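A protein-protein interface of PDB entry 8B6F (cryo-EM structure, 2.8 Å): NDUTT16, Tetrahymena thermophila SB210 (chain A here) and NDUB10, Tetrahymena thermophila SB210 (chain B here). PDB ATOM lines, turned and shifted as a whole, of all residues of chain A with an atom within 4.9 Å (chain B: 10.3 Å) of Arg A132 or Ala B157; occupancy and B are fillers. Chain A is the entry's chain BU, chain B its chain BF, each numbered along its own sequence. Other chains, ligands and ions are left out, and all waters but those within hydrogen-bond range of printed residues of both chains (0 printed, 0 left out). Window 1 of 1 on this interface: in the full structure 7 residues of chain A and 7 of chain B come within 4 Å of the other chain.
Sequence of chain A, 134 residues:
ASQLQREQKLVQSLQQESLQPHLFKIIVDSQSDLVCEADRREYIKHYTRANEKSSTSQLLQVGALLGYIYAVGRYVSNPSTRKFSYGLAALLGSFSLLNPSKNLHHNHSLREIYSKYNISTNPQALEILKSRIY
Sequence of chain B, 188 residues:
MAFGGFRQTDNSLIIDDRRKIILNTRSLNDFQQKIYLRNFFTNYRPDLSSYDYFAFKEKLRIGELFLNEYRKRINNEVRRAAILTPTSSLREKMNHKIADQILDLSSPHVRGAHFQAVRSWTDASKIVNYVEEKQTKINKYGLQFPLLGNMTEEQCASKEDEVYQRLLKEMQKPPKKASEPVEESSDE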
ATOM      1  N   ILE A  26      22.965  -2.604 -11.240  1.00  0.00           N
ATOM      2  CA  ILE A  26      23.282  -1.191 -11.048  1.00  0.00           C
ATOM      3  C   ILE A  26      22.230  -0.538 -10.161  1.00  0.00           C
ATOM      4  O   ILE A  26      22.556   0.246  -9.262  1.00  0.00           O
ATOM      5  CB  ILE A  26      23.403  -0.480 -12.409  1.00  0.00           C
ATOM      6  CG1 ILE A  26      24.630  -0.995 -13.165  1.00  0.00           C
ATOM      7  CG2 ILE A  26      23.494   1.034 -12.220  1.00  0.00           C
ATOM      8  CD1 ILE A  26      24.747  -0.478 -14.582  1.00  0.00           C
ATOM      9  N   SER A  30      22.718   1.199  -6.507  1.00  0.00           N
ATOM     10  CA  SER A  30      22.224   2.532  -6.188  1.00  0.00           C
ATOM     11  C   SER A  30      21.328   2.538  -4.958  1.00  0.00           C
ATOM     12  O   SER A  30      21.173   3.588  -4.325  1.00  0.00           O
ATOM     13  CB  SER A  30      21.454   3.099  -7.378  1.00  0.00           C
ATOM     14  OG  SER A  30      20.177   2.494  -7.475  1.00  0.00           O
ATOM     15  N   ILE A 128      17.051   6.305 -12.414  1.00  0.00           N
ATOM     16  CA  ILE A 128      18.168   5.757 -11.648  1.00  0.00           C
ATOM     17  C   ILE A 128      19.350   5.466 -12.562  1.00  0.00           C
ATOM     18  O   ILE A 128      20.499   5.787 -12.237  1.00  0.00           O
ATOM     19  CB  ILE A 128      17.703   4.489 -10.915  1.00  0.00           C
ATOM     20  CG1 ILE A 128      16.601   4.832  -9.915  1.00  0.00           C
ATOM     21  CG2 ILE A 128      18.865   3.831 -10.196  1.00  0.00           C
ATOM     22  CD1 ILE A 128      15.699   3.665  -9.591  1.00  0.00           C
ATOM     23  N   LEU A 129      19.092   4.848 -13.716  1.00  0.00           N
ATOM     24  CA  LEU A 129      20.181   4.456 -14.603  1.00  0.00           C
ATOM     25  C   LEU A 129      20.881   5.667 -15.208  1.00  0.00           C
ATOM     26  O   LEU A 129      22.108   5.669 -15.356  1.00  0.00           O
ATOM     27  CB  LEU A 129      19.663   3.530 -15.706  1.00  0.00           C
ATOM     28  CG  LEU A 129      19.671   2.014 -15.461  1.00  0.00           C
ATOM     29  CD1 LEU A 129      21.070   1.502 -15.143  1.00  0.00           C
ATOM     30  CD2 LEU A 129      18.709   1.616 -14.364  1.00  0.00           C
ATOM     31  N   LYS A 130      20.119   6.705 -15.567  1.00  0.00           N
ATOM     32  CA  LYS A 130      20.703   7.836 -16.285  1.00  0.00           C
ATOM     33  C   LYS A 130      21.881   8.432 -15.526  1.00  0.00           C
ATOM     34  O   LYS A 130      22.871   8.855 -16.135  1.00  0.00           O
ATOM     35  CB  LYS A 130      19.639   8.904 -16.540  1.00  0.00           C
ATOM     36  CG  LYS A 130      18.756   8.616 -17.746  1.00  0.00           C
ATOM     37  CD  LYS A 130      17.792   9.759 -18.032  1.00  0.00           C
ATOM     38  CE  LYS A 130      16.754   9.909 -16.932  1.00  0.00           C
ATOM     39  NZ  LYS A 130      15.752  10.963 -17.260  1.00  0.00           N
ATOM     40  N   SER A 131      21.795   8.477 -14.199  1.00  0.00           N
ATOM     41  CA  SER A 131      22.887   9.001 -13.392  1.00  0.00           C
ATOM     42  C   SER A 131      24.040   8.016 -13.237  1.00  0.00           C
ATOM     43  O   SER A 131      25.124   8.425 -12.810  1.00  0.00           O
ATOM     44  CB  SER A 131      22.366   9.398 -12.009  1.00  0.00           C
ATOM     45  OG  SER A 131      23.422   9.862 -11.184  1.00  0.00           O
ATOM     46  N   ARG A 132      23.837   6.744 -13.572  1.00  0.00           N
ATOM     47  CA  ARG A 132      24.835   5.696 -13.359  1.00  0.00           C
ATOM     48  C   ARG A 132      24.987   4.894 -14.649  1.00  0.00           C
ATOM     49  O   ARG A 132      24.207   3.974 -14.910  1.00  0.00           O
ATOM     50  CB  ARG A 132      24.435   4.794 -12.196  1.00  0.00           C
ATOM     51  CG  ARG A 132      24.205   5.537 -10.893  1.00  0.00           C
ATOM     52  CD  ARG A 132      23.378   4.712  -9.928  1.00  0.00           C
ATOM     53  NE  ARG A 132      23.162   5.414  -8.669  1.00  0.00           N
ATOM     54  CZ  ARG A 132      22.205   6.308  -8.461  1.00  0.00           C
ATOM     55  NH1 ARG A 132      21.355   6.646  -9.416  1.00  0.00           N
ATOM     56  NH2 ARG A 132      22.099   6.878  -7.265  1.00  0.00           N
ATOM     57  N   ILE A 133      25.991   5.236 -15.450  1.00  0.00           N
ATOM     58  CA  ILE A 133      26.292   4.531 -16.689  1.00  0.00           C
ATOM     59  C   ILE A 133      27.786   4.251 -16.720  1.00  0.00           C
ATOM     60  O   ILE A 133      28.594   5.144 -16.440  1.00  0.00           O
ATOM     61  CB  ILE A 133      25.876   5.344 -17.929  1.00  0.00           C
ATOM     62  CG1 ILE A 133      24.389   5.699 -17.860  1.00  0.00           C
ATOM     63  CG2 ILE A 133      26.181   4.559 -19.203  1.00  0.00           C
ATOM     64  CD1 ILE A 133      23.916   6.582 -19.004  1.00  0.00           C
ATOM     65  N   TYR A 134      28.154   3.019 -17.056  1.00  0.00           N
ATOM     66  CA  TYR A 134      29.560   2.649 -17.151  1.00  0.00           C
ATOM     67  C   TYR A 134      29.721   1.336 -17.907  1.00  0.00           C
ATOM     68  O   TYR A 134      30.787   1.044 -18.445  1.00  0.00           O
ATOM     69  CB  TYR A 134      30.186   2.534 -15.760  1.00  0.00           C
ATOM     70  CG  TYR A 134      29.628   1.405 -14.926  1.00  0.00           C
ATOM     71  CD1 TYR A 134      28.489   1.583 -14.155  1.00  0.00           C
ATOM     72  CD2 TYR A 134      30.245   0.162 -14.907  1.00  0.00           C
ATOM     73  CE1 TYR A 134      27.977   0.555 -13.391  1.00  0.00           C
ATOM     74  CE2 TYR A 134      29.741  -0.873 -14.146  1.00  0.00           C
ATOM     75  CZ  TYR A 134      28.606  -0.670 -13.390  1.00  0.00           C
ATOM     76  OH  TYR A 134      28.101  -1.698 -12.630  1.00  0.00           O
ATOM     77  OXT TYR A 134      28.788   0.538 -17.998  1.00  0.00           O
ATOM     78  N   GLY B 142      37.122  14.389  -8.396  1.00  0.00           N
ATOM     79  CA  GLY B 142      37.177  12.942  -8.315  1.00  0.00           C
ATOM     80  C   GLY B 142      38.414  12.340  -8.943  1.00  0.00           C
ATOM     81  O   GLY B 142      38.314  11.346  -9.670  1.00  0.00           O
ATOM     82  N   PHE B 145      40.105   8.195  -7.525  1.00  0.00           N
ATOM     83  CA  PHE B 145      39.475   6.878  -7.605  1.00  0.00           C
ATOM     84  C   PHE B 145      40.509   5.768  -7.522  1.00  0.00           C
ATOM     85  O   PHE B 145      40.481   4.985  -6.557  1.00  0.00           O
ATOM     86  CB  PHE B 145      38.636   6.761  -8.878  1.00  0.00           C
ATOM     87  CG  PHE B 145      38.460   5.342  -9.347  1.00  0.00           C
ATOM     88  CD1 PHE B 145      37.946   4.379  -8.494  1.00  0.00           C
ATOM     89  CD2 PHE B 145      38.792   4.973 -10.640  1.00  0.00           C
ATOM     90  CE1 PHE B 145      37.781   3.077  -8.915  1.00  0.00           C
ATOM     91  CE2 PHE B 145      38.629   3.669 -11.067  1.00  0.00           C
ATOM     92  CZ  PHE B 145      38.124   2.720 -10.203  1.00  0.00           C
ATOM     93  N   MET B 151      36.564   2.772  -4.535  1.00  0.00           N
ATOM     94  CA  MET B 151      35.134   2.943  -4.737  1.00  0.00           C
ATOM     95  C   MET B 151      34.610   1.793  -5.582  1.00  0.00           C
ATOM     96  O   MET B 151      35.363   1.126  -6.296  1.00  0.00           O
ATOM     97  CB  MET B 151      34.818   4.280  -5.415  1.00  0.00           C
ATOM     98  CG  MET B 151      35.313   5.495  -4.649  1.00  0.00           C
ATOM     99  SD  MET B 151      34.654   7.046  -5.289  1.00  0.00           S
ATOM    100  CE  MET B 151      35.195   6.978  -6.992  1.00  0.00           C
ATOM    101  N   THR B 152      33.302   1.569  -5.493  1.00  0.00           N
ATOM    102  CA  THR B 152      32.638   0.547  -6.282  1.00  0.00           C
ATOM    103  C   THR B 152      32.239   1.117  -7.641  1.00  0.00           C
ATOM    104  O   THR B 152      32.427   2.300  -7.929  1.00  0.00           O
ATOM    105  CB  THR B 152      31.420   0.000  -5.540  1.00  0.00           C
ATOM    106  OG1 THR B 152      30.466   1.051  -5.334  1.00  0.00           O
ATOM    107  CG2 THR B 152      31.826  -0.579  -4.197  1.00  0.00           C
ATOM    108  N   GLU B 153      31.670   0.262  -8.493  1.00  0.00           N
ATOM    109  CA  GLU B 153      31.288   0.701  -9.831  1.00  0.00           C
ATOM    110  C   GLU B 153      30.180   1.743  -9.777  1.00  0.00           C
ATOM    111  O   GLU B 153      30.237   2.754 -10.487  1.00  0.00           O
ATOM    112  CB  GLU B 153      30.852  -0.491 -10.678  1.00  0.00           C
ATOM    113  CG  GLU B 153      31.963  -1.470 -11.017  1.00  0.00           C
ATOM    114  CD  GLU B 153      32.340  -2.368  -9.857  1.00  0.00           C
ATOM    115  OE1 GLU B 153      31.873  -2.114  -8.727  1.00  0.00           O
ATOM    116  OE2 GLU B 153      33.097  -3.335 -10.077  1.00  0.00           O
ATOM    117  N   GLU B 154      29.160   1.516  -8.948  1.00  0.00           N
ATOM    118  CA  GLU B 154      28.081   2.490  -8.823  1.00  0.00           C
ATOM    119  C   GLU B 154      28.606   3.807  -8.271  1.00  0.00           C
ATOM    120  O   GLU B 154      28.209   4.885  -8.730  1.00  0.00           O
ATOM    121  CB  GLU B 154      26.969   1.930  -7.935  1.00  0.00           C
ATOM    122  CG  GLU B 154      25.776   2.864  -7.756  1.00  0.00           C
ATOM    123  CD  GLU B 154      25.945   3.844  -6.609  1.00  0.00           C
ATOM    124  OE1 GLU B 154      26.961   3.758  -5.889  1.00  0.00           O
ATOM    125  OE2 GLU B 154      25.057   4.703  -6.426  1.00  0.00           O
ATOM    126  N   GLN B 155      29.496   3.742  -7.281  1.00  0.00           N
ATOM    127  CA  GLN B 155      30.097   4.959  -6.751  1.00  0.00           C
ATOM    128  C   GLN B 155      30.876   5.696  -7.830  1.00  0.00           C
ATOM    129  O   GLN B 155      30.803   6.926  -7.929  1.00  0.00           O
ATOM    130  CB  GLN B 155      31.006   4.624  -5.570  1.00  0.00           C
ATOM    131  CG  GLN B 155      30.269   4.057  -4.371  1.00  0.00           C
ATOM    132  CD  GLN B 155      31.206   3.665  -3.250  1.00  0.00           C
ATOM    133  OE1 GLN B 155      32.399   3.952  -3.294  1.00  0.00           O
ATOM    134  NE2 GLN B 155      30.667   2.999  -2.235  1.00  0.00           N
ATOM    135  N   CYS B 156      31.632   4.963  -8.649  1.00  0.00           N
ATOM    136  CA  CYS B 156      32.394   5.602  -9.715  1.00  0.00           C
ATOM    137  C   CYS B 156      31.472   6.281 -10.719  1.00  0.00           C
ATOM    138  O   CYS B 156      31.740   7.406 -11.157  1.00  0.00           O
ATOM    139  CB  CYS B 156      33.281   4.575 -10.417  1.00  0.00           C
ATOM    140  SG  CYS B 156      34.553   3.850  -9.366  1.00  0.00           S
ATOM    141  N   ALA B 157      30.380   5.616 -11.095  1.00  0.00           N
ATOM    142  CA  ALA B 157      29.451   6.214 -12.047  1.00  0.00           C
ATOM    143  C   ALA B 157      28.802   7.465 -11.469  1.00  0.00           C
ATOM    144  O   ALA B 157      28.694   8.489 -12.153  1.00  0.00           O
ATOM    145  CB  ALA B 157      28.389   5.195 -12.457  1.00  0.00           C
ATOM    146  N   SER B 158      28.363   7.403 -10.211  1.00  0.00           N
ATOM    147  CA  SER B 158      27.757   8.575  -9.587  1.00  0.00           C
ATOM    148  C   SER B 158      28.753   9.722  -9.497  1.00  0.00           C
ATOM    149  O   SER B 158      28.401  10.883  -9.733  1.00  0.00           O
ATOM    150  CB  SER B 158      27.229   8.220  -8.198  1.00  0.00           C
ATOM    151  OG  SER B 158      26.240   7.208  -8.272  1.00  0.00           O
ATOM    152  N   LYS B 159      30.003   9.416  -9.147  1.00  0.00           N
ATOM    153  CA  LYS B 159      31.024  10.455  -9.070  1.00  0.00           C
ATOM    154  C   LYS B 159      31.304  11.059 -10.440  1.00  0.00           C
ATOM    155  O   LYS B 159      31.490  12.274 -10.558  1.00  0.00           O
ATOM    156  CB  LYS B 159      32.306   9.883  -8.464  1.00  0.00           C
ATOM    157  CG  LYS B 159      33.361  10.929  -8.118  1.00  0.00           C
ATOM    158  CD  LYS B 159      32.890  11.853  -7.005  1.00  0.00           C
ATOM    159  CE  LYS B 159      33.969  12.847  -6.610  1.00  0.00           C
ATOM    160  NZ  LYS B 159      33.503  13.765  -5.534  1.00  0.00           N
ATOM    161  N   GLU B 160      31.320  10.236 -11.492  1.00  0.00           N
ATOM    162  CA  GLU B 160      31.520  10.771 -12.835  1.00  0.00           C
ATOM    163  C   GLU B 160      30.405  11.738 -13.206  1.00  0.00           C
ATOM    164  O   GLU B 160      30.662  12.818 -13.749  1.00  0.00           O
ATOM    165  CB  GLU B 160      31.596   9.633 -13.854  1.00  0.00           C
ATOM    166  CG  GLU B 160      31.916  10.101 -15.270  1.00  0.00           C
ATOM    167  CD  GLU B 160      31.672   9.029 -16.315  1.00  0.00           C
ATOM    168  OE1 GLU B 160      31.216   7.929 -15.946  1.00  0.00           O
ATOM    169  OE2 GLU B 160      31.930   9.287 -17.508  1.00  0.00           O
ATOM    170  N   ASP B 161      29.156  11.367 -12.926  1.00  0.00           N
ATOM    171  CA  ASP B 161      28.046  12.263 -13.229  1.00  0.00           C
ATOM    172  C   ASP B 161      28.160  13.554 -12.430  1.00  0.00           C
ATOM    173  O   ASP B 161      27.938  14.647 -12.962  1.00  0.00           O
ATOM    174  CB  ASP B 161      26.717  11.568 -12.940  1.00  0.00           C
ATOM    175  CG  ASP B 161      25.522  12.435 -13.281  1.00  0.00           C
ATOM    176  OD1 ASP B 161      25.313  12.715 -14.480  1.00  0.00           O
ATOM    177  OD2 ASP B 161      24.792  12.838 -12.352  1.00  0.00           O
ATOM    178  N   GLU B 162      28.504  13.445 -11.145  1.00  0.00           N
ATOM    179  CA  GLU B 162      28.648  14.631 -10.310  1.00  0.00           C
ATOM    180  C   GLU B 162      29.749  15.544 -10.836  1.00  0.00           C
ATOM    181  O   GLU B 162      29.574  16.766 -10.902  1.00  0.00           O
ATOM    182  CB  GLU B 162      28.939  14.213  -8.869  1.00  0.00           C
ATOM    183  CG  GLU B 162      29.178  15.371  -7.917  1.00  0.00           C
ATOM    184  CD  GLU B 162      29.495  14.902  -6.512  1.00  0.00           C
ATOM    185  OE1 GLU B 162      29.419  13.681  -6.263  1.00  0.00           O
ATOM    186  OE2 GLU B 162      29.821  15.753  -5.658  1.00  0.00           O
ATOM    187  N   VAL B 163      30.891  14.969 -11.214  1.00  0.00           N
ATOM    188  CA  VAL B 163      32.003  15.774 -11.712  1.00  0.00           C
ATOM    189  C   VAL B 163      31.637  16.417 -13.042  1.00  0.00           C
ATOM    190  O   VAL B 163      32.010  17.563 -13.316  1.00  0.00           O
ATOM    191  CB  VAL B 163      33.274  14.913 -11.824  1.00  0.00           C
ATOM    192  CG1 VAL B 163      34.398  15.686 -12.500  1.00  0.00           C
ATOM    193  CG2 VAL B 163      33.715  14.453 -10.446  1.00  0.00           C
ATOM    194  N   TYR B 164      30.899  15.697 -13.886  1.00  0.00           N
ATOM    195  CA  TYR B 164      30.445  16.271 -15.146  1.00  0.00           C
ATOM    196  C   TYR B 164      29.557  17.484 -14.902  1.00  0.00           C
ATOM    197  O   TYR B 164      29.733  18.533 -15.529  1.00  0.00           O
ATOM    198  CB  TYR B 164      29.709  15.201 -15.952  1.00  0.00           C
ATOM    199  CG  TYR B 164      28.948  15.717 -17.146  1.00  0.00           C
ATOM    200  CD1 TYR B 164      29.584  15.977 -18.354  1.00  0.00           C
ATOM    201  CD2 TYR B 164      27.578  15.919 -17.069  1.00  0.00           C
ATOM    202  CE1 TYR B 164      28.871  16.438 -19.448  1.00  0.00           C
ATOM    203  CE2 TYR B 164      26.862  16.377 -18.148  1.00  0.00           C
ATOM    204  CZ  TYR B 164      27.509  16.636 -19.331  1.00  0.00           C
ATOM    205  OH  TYR B 164      26.768  17.090 -20.392  1.00  0.00           O
ATOM    206  N   GLN B 165      28.597  17.363 -13.983  1.00  0.00           N
ATOM    207  CA  GLN B 165      27.735  18.498 -13.671  1.00  0.00           C
ATOM    208  C   GLN B 165      28.544  19.665 -13.118  1.00  0.00           C
ATOM    209  O   GLN B 165      28.321  20.821 -13.495  1.00  0.00           O
ATOM    210  CB  GLN B 165      26.652  18.079 -12.679  1.00  0.00           C
ATOM    211  CG  GLN B 165      25.656  17.074 -13.234  1.00  0.00           C
ATOM    212  CD  GLN B 165      24.820  17.643 -14.360  1.00  0.00           C
ATOM    213  OE1 GLN B 165      24.869  18.838 -14.644  1.00  0.00           O
ATOM    214  NE2 GLN B 165      24.045  16.784 -15.013  1.00  0.00           N
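O of Glu B154 is in hydrogen-bond range of OG of Ser B158 (3.1 Å). NH1 of Arg A132 lies within hydrogen-bond range of O of Ile A128 (3.1 Å).
The side-chain carboxylate (OE2) of Glu B154 is in salt-bridge range of the guanidinium group (NE) of Arg A132 (3.0 Å). The side-chain hydroxyl of Ser A131 lies within hydrogen-bond range of the side-chain carboxylate of Asp B161 (3.5 Å).
Hydrophobic or aromatic side chains of chain B within 4 Å of the printed part of chain A: Ala B157. Among the printed residues, Asp or Glu carboxylates within 4 Å of a Lys or Arg side-chain nitrogen of the other chain: Arg A132 with Glu B154.
Among the printed residues, merely in contact across the chains: Ser A30 with Glu B154, Ser A131 with Ala B157, Arg A132 with Ala B157, Arg A132 with Ser B158, Ile A133 with Ala B157, Ile A133 with Glu B160, Tyr A134 with Glu B153 and Tyr A134 with Ala B157.
Arg A132 touches just these residues of chain B: Glu B154, Ala B157 and Ser B158. Of the printed residues of chain A, Ala B157 touches Ser A131, Arg A132, Ile A133 and Tyr A134. Ser A30 touches one residue of chain B. Ile A133 touches just these residues of chain B: Ala B157 (3.8 Å) and Glu B160 (3.9 Å). Of the printed residues of chain B, Tyr A134 touches Glu B153 (3.5 Å) and Ala B157 (3.99 Å). Printed residues of chain A within 4 Å of Asp B161: Ser A131 (3.5 Å). Printed residues of chain A within 4 Å of Glu B160: Ile A133 (3.9 Å). Printed residues of chain A within 4 Å of Glu B153: Tyr A134. Printed residues of chain A within 4 Å of Ser B158: Arg A132. Ile A26 touches none of the printed residues of chain B. Gln B155 touches none of the printed residues of chain A. The nearest residue of chain B that does not touch Arg A132 is Asp B161 (5.7 Å). The nearest printed residue of chain A that does not touch Ala B157 is Ile A26 (6.4 Å).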
